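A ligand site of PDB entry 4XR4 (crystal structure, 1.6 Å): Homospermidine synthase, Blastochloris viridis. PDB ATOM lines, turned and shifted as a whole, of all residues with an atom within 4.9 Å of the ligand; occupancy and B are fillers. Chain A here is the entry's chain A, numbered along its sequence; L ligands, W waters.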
ATOM      1  N   ILE A  15       3.555  11.870   3.362  1.00  0.00           N
ATOM      2  CA  ILE A  15       4.242  13.100   3.011  1.00  0.00           C
ATOM      3  C   ILE A  15       4.954  13.605   4.245  1.00  0.00           C
ATOM      4  O   ILE A  15       4.306  13.972   5.230  1.00  0.00           O
ATOM      5  CB  ILE A  15       3.290  14.171   2.482  1.00  0.00           C
ATOM      6  CG1 ILE A  15       2.356  13.583   1.417  1.00  0.00           C
ATOM      7  CG2 ILE A  15       4.106  15.326   1.955  1.00  0.00           C
ATOM      8  CD1 ILE A  15       1.327  14.594   0.866  1.00  0.00           C
ATOM      9  N   GLY A  16       6.276  13.600   4.199  1.00  0.00           N
ATOM     10  CA  GLY A  16       7.073  14.014   5.351  1.00  0.00           C
ATOM     11  C   GLY A  16       7.632  12.841   6.110  1.00  0.00           C
ATOM     12  O   GLY A  16       6.907  11.911   6.489  1.00  0.00           O
ATOM     13  N   PHE A  17       8.944  12.867   6.354  1.00  0.00           N
ATOM     14  CA  PHE A  17       9.622  11.828   7.123  1.00  0.00           C
ATOM     15  C   PHE A  17      10.577  12.501   8.100  1.00  0.00           C
ATOM     16  O   PHE A  17      11.779  12.175   8.152  1.00  0.00           O
ATOM     17  CB  PHE A  17      10.341  10.853   6.190  1.00  0.00           C
ATOM     18  CG  PHE A  17      10.594   9.500   6.781  1.00  0.00           C
ATOM     19  CD1 PHE A  17       9.543   8.727   7.235  1.00  0.00           C
ATOM     20  CD2 PHE A  17      11.872   9.000   6.889  1.00  0.00           C
ATOM     21  CE1 PHE A  17       9.758   7.487   7.761  1.00  0.00           C
ATOM     22  CE2 PHE A  17      12.092   7.747   7.410  1.00  0.00           C
ATOM     23  CZ  PHE A  17      11.041   6.989   7.845  1.00  0.00           C
ATOM     24  N   GLY A  18      10.031  13.464   8.840  1.00  0.00           N
ATOM     25  CA  GLY A  18      10.710  14.094   9.952  1.00  0.00           C
ATOM     26  C   GLY A  18      10.406  13.313  11.215  1.00  0.00           C
ATOM     27  O   GLY A  18      10.160  12.109  11.149  1.00  0.00           O
ATOM     28  N   SER A  19      10.410  13.978  12.365  1.00  0.00           N
ATOM     29  CA  SER A  19      10.288  13.251  13.614  1.00  0.00           C
ATOM     30  C   SER A  19       8.957  12.492  13.689  1.00  0.00           C
ATOM     31  O   SER A  19       8.924  11.381  14.175  1.00  0.00           O
ATOM     32  CB  SER A  19      10.468  14.182  14.845  1.00  0.00           C
ATOM     33  OG  SER A  19       9.294  14.865  15.255  1.00  0.00           O
ATOM     34  N   ILE A  20       7.883  13.065  13.170  1.00  0.00           N
ATOM     35  CA  ILE A  20       6.595  12.364  13.281  1.00  0.00           C
ATOM     36  C   ILE A  20       6.466  11.248  12.255  1.00  0.00           C
ATOM     37  O   ILE A  20       6.038  10.158  12.563  1.00  0.00           O
ATOM     38  CB  ILE A  20       5.447  13.363  13.168  1.00  0.00           C
ATOM     39  CG1 ILE A  20       5.601  14.409  14.286  1.00  0.00           C
ATOM     40  CG2 ILE A  20       4.100  12.623  13.262  1.00  0.00           C
ATOM     41  CD1 ILE A  20       5.869  13.853  15.680  1.00  0.00           C
ATOM     42  N   GLY A  21       6.855  11.515  11.014  1.00  0.00           N
ATOM     43  CA  GLY A  21       6.820  10.475  10.003  1.00  0.00           C
ATOM     44  C   GLY A  21       7.640   9.262  10.393  1.00  0.00           C
ATOM     45  O   GLY A  21       7.212   8.111  10.212  1.00  0.00           O
ATOM     46  N   ILE A  42       7.423  10.529   0.891  1.00  0.00           N
ATOM     47  CA  ILE A  42       7.893  11.663   0.109  1.00  0.00           C
ATOM     48  C   ILE A  42       8.485  12.721   1.031  1.00  0.00           C
ATOM     49  O   ILE A  42       7.795  13.233   1.920  1.00  0.00           O
ATOM     50  CB  ILE A  42       6.759  12.313  -0.722  1.00  0.00           C
ATOM     51  CG1 ILE A  42       6.039  11.258  -1.559  1.00  0.00           C
ATOM     52  CG2 ILE A  42       7.299  13.414  -1.609  1.00  0.00           C
ATOM     53  CD1 ILE A  42       4.747  11.750  -2.163  1.00  0.00           C
ATOM     54  N   ASP A  43       9.762  13.031   0.853  1.00  0.00           N
ATOM     55  CA  ASP A  43      10.403  14.057   1.666  1.00  0.00           C
ATOM     56  C   ASP A  43      11.665  14.548   0.921  1.00  0.00           C
ATOM     57  O   ASP A  43      12.387  13.734   0.394  1.00  0.00           O
ATOM     58  CB  ASP A  43      10.748  13.469   3.028  1.00  0.00           C
ATOM     59  CG  ASP A  43      11.209  14.512   4.042  1.00  0.00           C
ATOM     60  OD1 ASP A  43      12.191  15.246   3.766  1.00  0.00           O
ATOM     61  OD2 ASP A  43      10.609  14.558   5.139  1.00  0.00           O
ATOM     62  N   PRO A  44      11.907  15.861   0.895  1.00  0.00           N
ATOM     63  CA  PRO A  44      13.097  16.345   0.163  1.00  0.00           C
ATOM     64  C   PRO A  44      14.436  16.153   0.864  1.00  0.00           C
ATOM     65  O   PRO A  44      15.483  16.369   0.256  1.00  0.00           O
ATOM     66  CB  PRO A  44      12.810  17.839  -0.002  1.00  0.00           C
ATOM     67  CG  PRO A  44      11.968  18.169   1.210  1.00  0.00           C
ATOM     68  CD  PRO A  44      11.079  16.962   1.375  1.00  0.00           C
ATOM     69  N   SER A  45      14.420  15.735   2.132  1.00  0.00           N
ATOM     70  CA  SER A  45      15.643  15.688   2.933  1.00  0.00           C
ATOM     71  C   SER A  45      16.552  14.478   2.675  1.00  0.00           C
ATOM     72  O   SER A  45      16.092  13.348   2.649  1.00  0.00           O
ATOM     73  CB  SER A  45      15.286  15.710   4.426  1.00  0.00           C
ATOM     74  OG  SER A  45      16.321  15.169   5.224  1.00  0.00           O
ATOM     75  N   ALA A  48      16.478  12.261   5.713  1.00  0.00           N
ATOM     76  CA  ALA A  48      15.265  11.438   5.707  1.00  0.00           C
ATOM     77  C   ALA A  48      15.405  10.253   4.751  1.00  0.00           C
ATOM     78  O   ALA A  48      15.027   9.109   5.082  1.00  0.00           O
ATOM     79  CB  ALA A  48      14.053  12.299   5.332  1.00  0.00           C
ATOM     80  N   GLN A  62      11.525  14.469  -2.859  1.00  0.00           N
ATOM     81  CA  GLN A  62      10.967  15.611  -3.550  1.00  0.00           C
ATOM     82  C   GLN A  62      10.180  16.470  -2.579  1.00  0.00           C
ATOM     83  O   GLN A  62       9.481  15.959  -1.711  1.00  0.00           O
ATOM     84  CB  GLN A  62      10.070  15.125  -4.710  1.00  0.00           C
ATOM     85  CG  GLN A  62       9.473  16.226  -5.577  1.00  0.00           C
ATOM     86  CD  GLN A  62      10.538  17.068  -6.240  1.00  0.00           C
ATOM     87  OE1 GLN A  62      10.447  18.298  -6.281  1.00  0.00           O
ATOM     88  NE2 GLN A  62      11.571  16.416  -6.751  1.00  0.00           N
ATOM     89  N   ALA A  63      10.354  17.775  -2.697  1.00  0.00           N
ATOM     90  CA  ALA A  63       9.474  18.715  -2.012  1.00  0.00           C
ATOM     91  C   ALA A  63       8.129  18.804  -2.740  1.00  0.00           C
ATOM     92  O   ALA A  63       8.091  19.012  -3.960  1.00  0.00           O
ATOM     93  CB  ALA A  63      10.130  20.059  -1.923  1.00  0.00           C
ATOM     94  N   VAL A  64       7.040  18.646  -2.002  1.00  0.00           N
ATOM     95  CA  VAL A  64       5.700  18.874  -2.557  1.00  0.00           C
ATOM     96  C   VAL A  64       5.435  20.371  -2.570  1.00  0.00           C
ATOM     97  O   VAL A  64       5.578  21.052  -1.572  1.00  0.00           O
ATOM     98  CB  VAL A  64       4.631  18.132  -1.751  1.00  0.00           C
ATOM     99  CG1 VAL A  64       3.260  18.366  -2.332  1.00  0.00           C
ATOM    100  CG2 VAL A  64       4.933  16.671  -1.709  1.00  0.00           C
ATOM    101  N   LEU A  89       2.383  14.401   7.021  1.00  0.00           N
ATOM    102  CA  LEU A  89       3.127  14.725   8.237  1.00  0.00           C
ATOM    103  C   LEU A  89       4.284  15.675   7.885  1.00  0.00           C
ATOM    104  O   LEU A  89       5.411  15.491   8.317  1.00  0.00           O
ATOM    105  CB  LEU A  89       3.663  13.443   8.877  1.00  0.00           C
ATOM    106  CG  LEU A  89       2.608  12.357   9.112  1.00  0.00           C
ATOM    107  CD1 LEU A  89       3.247  11.033   9.473  1.00  0.00           C
ATOM    108  CD2 LEU A  89       1.628  12.792  10.194  1.00  0.00           C
ATOM    109  N   SER A  90       3.975  16.722   7.111  1.00  0.00           N
ATOM    110  CA  SER A  90       5.002  17.589   6.542  1.00  0.00           C
ATOM    111  C   SER A  90       4.922  19.007   7.092  1.00  0.00           C
ATOM    112  O   SER A  90       3.992  19.359   7.804  1.00  0.00           O
ATOM    113  CB  SER A  90       4.860  17.625   5.002  1.00  0.00           C
ATOM    114  OG  SER A  90       3.605  18.132   4.597  1.00  0.00           O
ATOM    115  N   VAL A  91       5.910  19.819   6.732  1.00  0.00           N
ATOM    116  CA  VAL A  91       5.839  21.257   6.819  1.00  0.00           C
ATOM    117  C   VAL A  91       5.862  21.838   5.404  1.00  0.00           C
ATOM    118  O   VAL A  91       6.272  21.158   4.458  1.00  0.00           O
ATOM    119  CB  VAL A  91       7.029  21.843   7.630  1.00  0.00           C
ATOM    120  CG1 VAL A  91       7.032  21.323   9.052  1.00  0.00           C
ATOM    121  CG2 VAL A  91       8.369  21.507   6.957  1.00  0.00           C
ATOM    122  N   ASP A  92       5.413  23.084   5.285  1.00  0.00           N
ATOM    123  CA  ASP A  92       5.550  23.909   4.086  1.00  0.00           C
ATOM    124  C   ASP A  92       4.624  23.480   2.958  1.00  0.00           C
ATOM    125  O   ASP A  92       4.805  23.905   1.820  1.00  0.00           O
ATOM    126  CB  ASP A  92       7.004  23.914   3.600  1.00  0.00           C
ATOM    127  CG  ASP A  92       7.947  24.599   4.574  1.00  0.00           C
ATOM    128  OD1 ASP A  92       7.453  25.264   5.500  1.00  0.00           O
ATOM    129  OD2 ASP A  92       9.179  24.496   4.377  1.00  0.00           O
ATOM    130  N   THR A  93       3.638  22.657   3.284  1.00  0.00           N
ATOM    131  CA  THR A  93       2.680  22.173   2.304  1.00  0.00           C
ATOM    132  C   THR A  93       1.284  22.575   2.727  1.00  0.00           C
ATOM    133  O   THR A  93       0.993  22.697   3.904  1.00  0.00           O
ATOM    134  CB  THR A  93       2.692  20.640   2.156  1.00  0.00           C
ATOM    135  OG1 THR A  93       2.362  20.042   3.413  1.00  0.00           O
ATOM    136  CG2 THR A  93       4.071  20.152   1.717  1.00  0.00           C
ATOM    137  N   THR A 112      -1.885  16.590  10.833  1.00  0.00           N
ATOM    138  CA  THR A 112      -1.756  16.953  12.256  1.00  0.00           C
ATOM    139  C   THR A 112      -1.715  18.473  12.452  1.00  0.00           C
ATOM    140  O   THR A 112      -1.468  18.950  13.555  1.00  0.00           O
ATOM    141  CB  THR A 112      -0.479  16.322  12.881  1.00  0.00           C
ATOM    142  OG1 THR A 112       0.681  16.945  12.336  1.00  0.00           O
ATOM    143  CG2 THR A 112      -0.471  14.802  12.671  1.00  0.00           C
ATOM    144  N   VAL A 113      -1.979  19.226  11.408  1.00  0.00           N
ATOM    145  CA  VAL A 113      -1.874  20.680  11.427  1.00  0.00           C
ATOM    146  C   VAL A 113      -2.521  21.218  10.170  1.00  0.00           C
ATOM    147  O   VAL A 113      -2.546  20.524   9.151  1.00  0.00           O
ATOM    148  CB  VAL A 113      -0.410  21.137  11.498  1.00  0.00           C
ATOM    149  CG1 VAL A 113       0.373  20.580  10.310  1.00  0.00           C
ATOM    150  CG2 VAL A 113      -0.281  22.655  11.561  1.00  0.00           C
ATOM    151  N   GLU A 115      -1.529  23.370   7.709  1.00  0.00           N
ATOM    152  CA  GLU A 115      -0.283  23.986   7.249  1.00  0.00           C
ATOM    153  C   GLU A 115      -0.571  24.681   5.914  1.00  0.00           C
ATOM    154  O   GLU A 115      -1.381  24.194   5.121  1.00  0.00           O
ATOM    155  CB  GLU A 115       0.784  22.909   7.115  1.00  0.00           C
ATOM    156  CG  GLU A 115       2.179  23.338   6.667  1.00  0.00           C
ATOM    157  CD  GLU A 115       2.982  23.977   7.765  1.00  0.00           C
ATOM    158  OE1 GLU A 115       2.422  24.174   8.856  1.00  0.00           O
ATOM    159  OE2 GLU A 115       4.180  24.273   7.543  1.00  0.00           O
ATOM    160  N   GLY A 158      -3.111  14.856  15.486  1.00  0.00           N
ATOM    161  CA  GLY A 158      -1.888  14.463  16.167  1.00  0.00           C
ATOM    162  C   GLY A 158      -2.173  14.324  17.653  1.00  0.00           C
ATOM    163  O   GLY A 158      -3.268  13.910  18.051  1.00  0.00           O
ATOM    164  N   ALA A 159      -1.182  14.626  18.481  1.00  0.00           N
ATOM    165  CA  ALA A 159      -1.366  14.625  19.947  1.00  0.00           C
ATOM    166  C   ALA A 159      -2.168  15.848  20.394  1.00  0.00           C
ATOM    167  O   ALA A 159      -3.113  15.735  21.202  1.00  0.00           O
ATOM    168  CB  ALA A 159      -0.016  14.585  20.631  1.00  0.00           C
ATOM    169  N   ASN A 160      -1.791  17.007  19.880  1.00  0.00           N
ATOM    170  CA  ASN A 160      -2.426  18.263  20.202  1.00  0.00           C
ATOM    171  C   ASN A 160      -2.062  19.280  19.143  1.00  0.00           C
ATOM    172  O   ASN A 160      -0.938  19.800  19.156  1.00  0.00           O
ATOM    173  CB  ASN A 160      -2.023  18.762  21.611  1.00  0.00           C
ATOM    174  CG  ASN A 160      -0.501  18.883  21.848  1.00  0.00           C
ATOM    175  OD1 ASN A 160       0.294  18.044  21.443  1.00  0.00           O
ATOM    176  ND2 ASN A 160      -0.115  19.961  22.541  1.00  0.00           N
ATOM    177  N   PRO A 161      -2.988  19.563  18.220  1.00  0.00           N
ATOM    178  CA  PRO A 161      -4.365  19.084  18.121  1.00  0.00           C
ATOM    179  C   PRO A 161      -4.436  17.596  17.846  1.00  0.00           C
ATOM    180  O   PRO A 161      -3.575  17.022  17.203  1.00  0.00           O
ATOM    181  CB  PRO A 161      -4.930  19.852  16.924  1.00  0.00           C
ATOM    182  CG  PRO A 161      -3.699  20.248  16.100  1.00  0.00           C
ATOM    183  CD  PRO A 161      -2.650  20.524  17.136  1.00  0.00           C
ATOM    184  N   TRP A 227      10.510  17.834  18.883  1.00  0.00           N
ATOM    185  CA  TRP A 227       9.730  17.672  17.661  1.00  0.00           C
ATOM    186  C   TRP A 227      10.106  18.861  16.779  1.00  0.00           C
ATOM    187  O   TRP A 227      10.966  19.647  17.169  1.00  0.00           O
ATOM    188  CB  TRP A 227       8.229  17.590  17.953  1.00  0.00           C
ATOM    189  CG  TRP A 227       7.660  18.815  18.573  1.00  0.00           C
ATOM    190  CD1 TRP A 227       7.766  19.211  19.856  1.00  0.00           C
ATOM    191  CD2 TRP A 227       6.882  19.812  17.892  1.00  0.00           C
ATOM    192  NE1 TRP A 227       7.115  20.414  20.040  1.00  0.00           N
ATOM    193  CE2 TRP A 227       6.566  20.813  18.854  1.00  0.00           C
ATOM    194  CE3 TRP A 227       6.431  19.969  16.592  1.00  0.00           C
ATOM    195  CZ2 TRP A 227       5.787  21.927  18.540  1.00  0.00           C
ATOM    196  CZ3 TRP A 227       5.682  21.097  16.269  1.00  0.00           C
ATOM    197  CH2 TRP A 227       5.361  22.060  17.244  1.00  0.00           C
ATOM    198  N   SER A 228       9.526  18.966  15.589  1.00  0.00           N
ATOM    199  CA  SER A 228       9.848  20.018  14.615  1.00  0.00           C
ATOM    200  C   SER A 228      10.294  21.317  15.234  1.00  0.00           C
ATOM    201  O   SER A 228       9.539  21.956  15.960  1.00  0.00           O
ATOM    202  CB  SER A 228       8.640  20.357  13.739  1.00  0.00           C
ATOM    203  OG  SER A 228       9.049  21.040  12.550  1.00  0.00           O
ATOM    204  N   VAL A 229      11.505  21.744  14.896  1.00  0.00           N
ATOM    205  CA  VAL A 229      11.945  23.068  15.255  1.00  0.00           C
ATOM    206  C   VAL A 229      11.277  24.050  14.315  1.00  0.00           C
ATOM    207  O   VAL A 229      10.758  25.085  14.761  1.00  0.00           O
ATOM    208  CB  VAL A 229      13.471  23.196  15.220  1.00  0.00           C
ATOM    209  CG1 VAL A 229      13.877  24.660  15.341  1.00  0.00           C
ATOM    210  CG2 VAL A 229      14.082  22.372  16.330  1.00  0.00           C
ATOM    211  N   GLU A 230      11.248  23.734  13.019  1.00  0.00           N
ATOM    212  CA  GLU A 230      10.645  24.620  12.039  1.00  0.00           C
ATOM    213  C   GLU A 230       9.177  24.857  12.380  1.00  0.00           C
ATOM    214  O   GLU A 230       8.697  25.993  12.366  1.00  0.00           O
ATOM    215  CB  GLU A 230      10.793  24.061  10.626  1.00  0.00           C
ATOM    216  CG  GLU A 230      12.229  24.213  10.128  1.00  0.00           C
ATOM    217  CD  GLU A 230      12.449  23.752   8.690  1.00  0.00           C
ATOM    218  OE1 GLU A 230      11.585  23.040   8.130  1.00  0.00           O
ATOM    219  OE2 GLU A 230      13.501  24.097   8.125  1.00  0.00           O
ATOM    220  N   GLY A 231       8.469  23.792  12.737  1.00  0.00           N
ATOM    221  CA  GLY A 231       7.059  23.869  13.006  1.00  0.00           C
ATOM    222  C   GLY A 231       6.779  24.602  14.305  1.00  0.00           C
ATOM    223  O   GLY A 231       5.819  25.372  14.389  1.00  0.00           O
ATOM    224  N   TRP A 346      19.688  24.047  14.130  1.00  0.00           N
ATOM    225  CA  TRP A 346      18.716  23.465  15.052  1.00  0.00           C
ATOM    226  C   TRP A 346      18.870  21.968  15.112  1.00  0.00           C
ATOM    227  O   TRP A 346      19.503  21.365  14.244  1.00  0.00           O
ATOM    228  CB  TRP A 346      17.287  23.869  14.675  1.00  0.00           C
ATOM    229  CG  TRP A 346      16.825  23.523  13.289  1.00  0.00           C
ATOM    230  CD1 TRP A 346      16.756  24.369  12.226  1.00  0.00           C
ATOM    231  CD2 TRP A 346      16.320  22.251  12.828  1.00  0.00           C
ATOM    232  NE1 TRP A 346      16.258  23.703  11.113  1.00  0.00           N
ATOM    233  CE2 TRP A 346      15.998  22.399  11.459  1.00  0.00           C
ATOM    234  CE3 TRP A 346      16.136  20.997  13.431  1.00  0.00           C
ATOM    235  CZ2 TRP A 346      15.488  21.357  10.691  1.00  0.00           C
ATOM    236  CZ3 TRP A 346      15.641  19.953  12.662  1.00  0.00           C
ATOM    237  CH2 TRP A 346      15.319  20.137  11.305  1.00  0.00           C
ATOM    238  N   ILE A 348      16.625  18.277  16.573  1.00  0.00           N
ATOM    239  CA  ILE A 348      15.579  17.562  17.278  1.00  0.00           C
ATOM    240  C   ILE A 348      16.200  16.432  18.068  1.00  0.00           C
ATOM    241  O   ILE A 348      16.943  15.627  17.512  1.00  0.00           O
ATOM    242  CB  ILE A 348      14.525  17.019  16.300  1.00  0.00           C
ATOM    243  CG1 ILE A 348      13.825  18.187  15.592  1.00  0.00           C
ATOM    244  CG2 ILE A 348      13.536  16.136  17.002  1.00  0.00           C
ATOM    245  CD1 ILE A 348      12.934  17.774  14.432  1.00  0.00           C
ATOM    246  N   VAL A 398       2.100  11.651  19.277  1.00  0.00           N
ATOM    247  CA  VAL A 398       1.613  12.133  17.983  1.00  0.00           C
ATOM    248  C   VAL A 398       1.395  10.979  16.996  1.00  0.00           C
ATOM    249  O   VAL A 398       0.332  10.884  16.385  1.00  0.00           O
ATOM    250  CB  VAL A 398       2.574  13.148  17.350  1.00  0.00           C
ATOM    251  CG1 VAL A 398       2.030  13.686  16.040  1.00  0.00           C
ATOM    252  CG2 VAL A 398       2.858  14.282  18.303  1.00  0.00           C
HETATM  253  P1  LIG L   1      10.187  17.888  11.236  1.00  0.00           P
HETATM  254  O1  LIG L   1      10.985  16.911  12.020  1.00  0.00           O
HETATM  255  O2  LIG L   1      10.644  19.294  11.097  1.00  0.00           O
HETATM  256  O3  LIG L   1       9.946  17.275   9.777  1.00  0.00           O
HETATM  257  C1  LIG L   1       9.331  17.995   8.737  1.00  0.00           C
HETATM  258  C2  LIG L   1       9.644  17.214   7.500  1.00  0.00           C
HETATM  259  O4  LIG L   1       8.942  17.823   6.438  1.00  0.00           O
HETATM  260  C3  LIG L   1      11.131  17.283   7.161  1.00  0.00           C
HETATM  261  O5  LIG L   1      11.683  15.976   7.037  1.00  0.00           O
HETATM  262  C4  LIG L   1      11.183  18.083   5.877  1.00  0.00           C
HETATM  263  O6  LIG L   1      12.261  17.732   4.972  1.00  0.00           O
HETATM  264  C5  LIG L   1       9.809  17.800   5.302  1.00  0.00           C
HETATM  265  N1  LIG L   1       9.404  18.762   4.284  1.00  0.00           N
HETATM  266  C6  LIG L   1       9.774  20.057   4.192  1.00  0.00           C
HETATM  267  N2  LIG L   1       9.243  20.624   3.110  1.00  0.00           N
HETATM  268  C7  LIG L   1       8.533  19.671   2.494  1.00  0.00           C
HETATM  269  C8  LIG L   1       7.716  19.610   1.307  1.00  0.00           C
HETATM  270  N3  LIG L   1       7.571  20.710   0.574  1.00  0.00           N
HETATM  271  N4  LIG L   1       7.140  18.442   0.974  1.00  0.00           N
HETATM  272  C9  LIG L   1       7.295  17.355   1.723  1.00  0.00           C
HETATM  273  N5  LIG L   1       8.012  17.328   2.855  1.00  0.00           N
HETATM  274  C10 LIG L   1       8.638  18.450   3.261  1.00  0.00           C
HETATM  275  O7  LIG L   1       8.667  17.980  11.762  1.00  0.00           O
HETATM  276  P2  LIG L   1       7.833  16.881  12.588  1.00  0.00           P
HETATM  277  O8  LIG L   1       8.188  16.914  14.039  1.00  0.00           O
HETATM  278  O9  LIG L   1       7.870  15.554  11.869  1.00  0.00           O
HETATM  279  O10 LIG L   1       6.393  17.550  12.371  1.00  0.00           O
HETATM  280  C11 LIG L   1       5.728  17.320  11.122  1.00  0.00           C
HETATM  281  C12 LIG L   1       4.434  18.129  11.043  1.00  0.00           C
HETATM  282  O11 LIG L   1       3.584  17.720  12.097  1.00  0.00           O
HETATM  283  C13 LIG L   1       4.671  19.592  11.286  1.00  0.00           C
HETATM  284  O12 LIG L   1       3.815  20.356  10.439  1.00  0.00           O
HETATM  285  C14 LIG L   1       4.265  19.809  12.735  1.00  0.00           C
HETATM  286  O13 LIG L   1       3.780  21.109  12.970  1.00  0.00           O
HETATM  287  C15 LIG L   1       3.150  18.785  12.909  1.00  0.00           C
HETATM  288  N6  LIG L   1       2.990  18.272  14.279  1.00  0.00           N
HETATM  289  C16 LIG L   1       1.763  18.206  14.840  1.00  0.00           C
HETATM  290  C17 LIG L   1       1.638  17.720  16.144  1.00  0.00           C
HETATM  291  C18 LIG L   1       0.318  17.541  16.842  1.00  0.00           C
HETATM  292  O14 LIG L   1       0.350  17.005  17.929  1.00  0.00           O
HETATM  293  N7  LIG L   1      -0.812  17.883  16.244  1.00  0.00           N
HETATM  294  C19 LIG L   1       2.767  17.352  16.862  1.00  0.00           C
HETATM  295  C20 LIG L   1       4.009  17.411  16.249  1.00  0.00           C
HETATM  296  C21 LIG L   1       4.089  17.881  14.941  1.00  0.00           C
HETATM  297  O   HOH W   1      11.624  22.285   5.561  1.00  0.00           O
HETATM  298  O   HOH W   2      12.438  21.043  12.238  1.00  0.00           O
HETATM  299  O   HOH W   3       3.776  23.283  11.217  1.00  0.00           O
HETATM  300  O   HOH W   4       9.936  23.132   2.219  1.00  0.00           O
HETATM  301  O   HOH W   5      13.417  15.898  11.410  1.00  0.00           O
HETATM  302  O   HOH W   6      11.901  20.260   8.758  1.00  0.00           O
HETATM  303  O   HOH W   7       1.746  20.003  18.718  1.00  0.00           O
HETATM  304  O   HOH W   8       7.380  14.114   9.703  1.00  0.00           O
HETATM  305  O   HOH W   9       6.094  23.637  -0.551  1.00  0.00           O
HETATM  306  O   HOH W  10      14.196  19.725   4.819  1.00  0.00           O
HETATM  307  O   HOH W  11       8.766  23.430  -0.290  1.00  0.00           O
HETATM  308  O   HOH W  12       1.738  21.715  15.523  1.00  0.00           O
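The side-chain carboxylate (OD1) of Asp 43 lies within hydrogen-bond range of the backbone NH (N) of Ser 45, at 2.8 Å. N of Phe 17 is in hydrogen-bond range of OD2 of Asp 43, 2.7 Å away. The backbone carbonyl oxygen (O) of Asp 43 sits at hydrogen-bond distance from the backbone NH (N) of Gln 62 (3.4 Å). OG of Ser 228 sits at hydrogen-bond distance from N of Gly 231. The side-chain hydroxyl (OG1) of Thr 93 lies within hydrogen-bond range of the side-chain hydroxyl (OG) of Ser 90, 2.6 Å away. O of Ile 15 sits at hydrogen-bond distance from N of Ser 90 (3.3 Å). N of Leu 89 sits at hydrogen-bond distance from O of Ile 15, at 2.7 Å. The backbone NH (N) of Ala 48 sits at hydrogen-bond distance from the side-chain hydroxyl (OG) of Ser 45 (3.0 Å).
N2 of the ligand lies close to O of Val 91. Merely in contact with the ligand: Ile 348 (3.2 Å), Gly 18 (3.3 Å), Leu 89 (3.4 Å), Val 398 (3.4 Å), Pro 44 (3.4 Å), Val 113 (3.5 Å), Trp 227 (3.5 Å), Gly 158 (3.6 Å), Thr 93 (3.6 Å), Ala 63 (3.6 Å), Ser 45 (3.7 Å), Ile 15 (3.8 Å) and Phe 17 (3.8 Å). Hydrophobic or aromatic side chains that line the ligand: Ile 15, Ile 20, Pro 44, Ala 63, Val 64, Val 91, Val 113, Ala 159, Pro 161, Trp 227, Ile 348 and Val 398. 24 residues have an atom within 4 Å of the ligand: Ile 15, Phe 17, Gly 18, Ser 19, Ile 20, Asp 43, Pro 44, Ser 45, Ala 63, Val 64, Leu 89, Ser 90, Val 91, Thr 93, Thr 112, Val 113, Gly 158, Ala 159, Asn 160, Pro 161, Trp 227, Ser 228, Ile 348 and Val 398.
The side-chain carboxylate (OD2) of Asp 43 sits at hydrogen-bond distance from an oxygen (O5) of the ligand (2.6 Å). The backbone NH (N) of Ser 19 is in hydrogen-bond range of an oxygen (O1) of the ligand, 3.0 Å away. O8 of the ligand is in hydrogen-bond range of OG of Ser 19, 2.6 Å away. An oxygen (O8) of the ligand lies within hydrogen-bond range of the backbone NH (N) of Ser 228. The side-chain hydroxyl (OG) of Ser 228 lies within hydrogen-bond range of an oxygen (O2) of the ligand, 2.8 Å away. The backbone NH of Ile 20 sits at hydrogen-bond distance from an oxygen (O9) of the ligand, 2.8 Å away. O12 of the ligand is in hydrogen-bond range of O of Ser 90 (2.8 Å). An oxygen (O14) of the ligand lies within hydrogen-bond range of the backbone NH of Ala 159, at 2.9 Å. N of Asn 160 is in hydrogen-bond range of O14 of the ligand (2.9 Å). The backbone carbonyl oxygen (O) of Asn 160 lies close to a nitrogen (N7) of the ligand (3.5 Å). N of Val 64 lies within hydrogen-bond range of N4 of the ligand (3.0 Å). A nitrogen (N3) of the ligand sits at hydrogen-bond distance from the backbone carbonyl oxygen of Val 64, at 2.9 Å. O of Thr 112 is in hydrogen-bond range of N7 of the ligand. O11 of the ligand lies close to OG1 of Thr 112 (3.0 Å). A nitrogen (N7) of the ligand lies within hydrogen-bond range of the backbone carbonyl oxygen (O) of Pro 161, at 3.0 Å.
Water W8 lies within hydrogen-bond range of O9 of the ligand (2.6 Å), O of Leu 89 (2.8 Å), N of Gly 18 (2.9 Å) and N of Gly 21 (3.0 Å). Water W4 bridges the side-chain carboxylate of Asp 92 (2.7 Å) and a nitrogen (N2) of the ligand (2.8 Å). Water W2 lies within hydrogen-bond range of an oxygen (O2) of the ligand (2.8 Å), the backbone NH of Val 229 (2.9 Å), the backbone NH of Glu 230 (3.0 Å) and the side-chain hydroxyl of Ser 228 (3.4 Å). Water W3 lies within hydrogen-bond range of O13 of the ligand and OE1 of Glu 115. Water W6 lies within hydrogen-bond range of an oxygen (O2) of the ligand (2.8 Å) and the side-chain carboxylate (OE1) of Glu 230 (2.9 Å). Water W9 lies within hydrogen-bond range of O of Asp 92 (2.7 Å), O of Val 64 (2.8 Å) and N3 of the ligand (3.5 Å).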
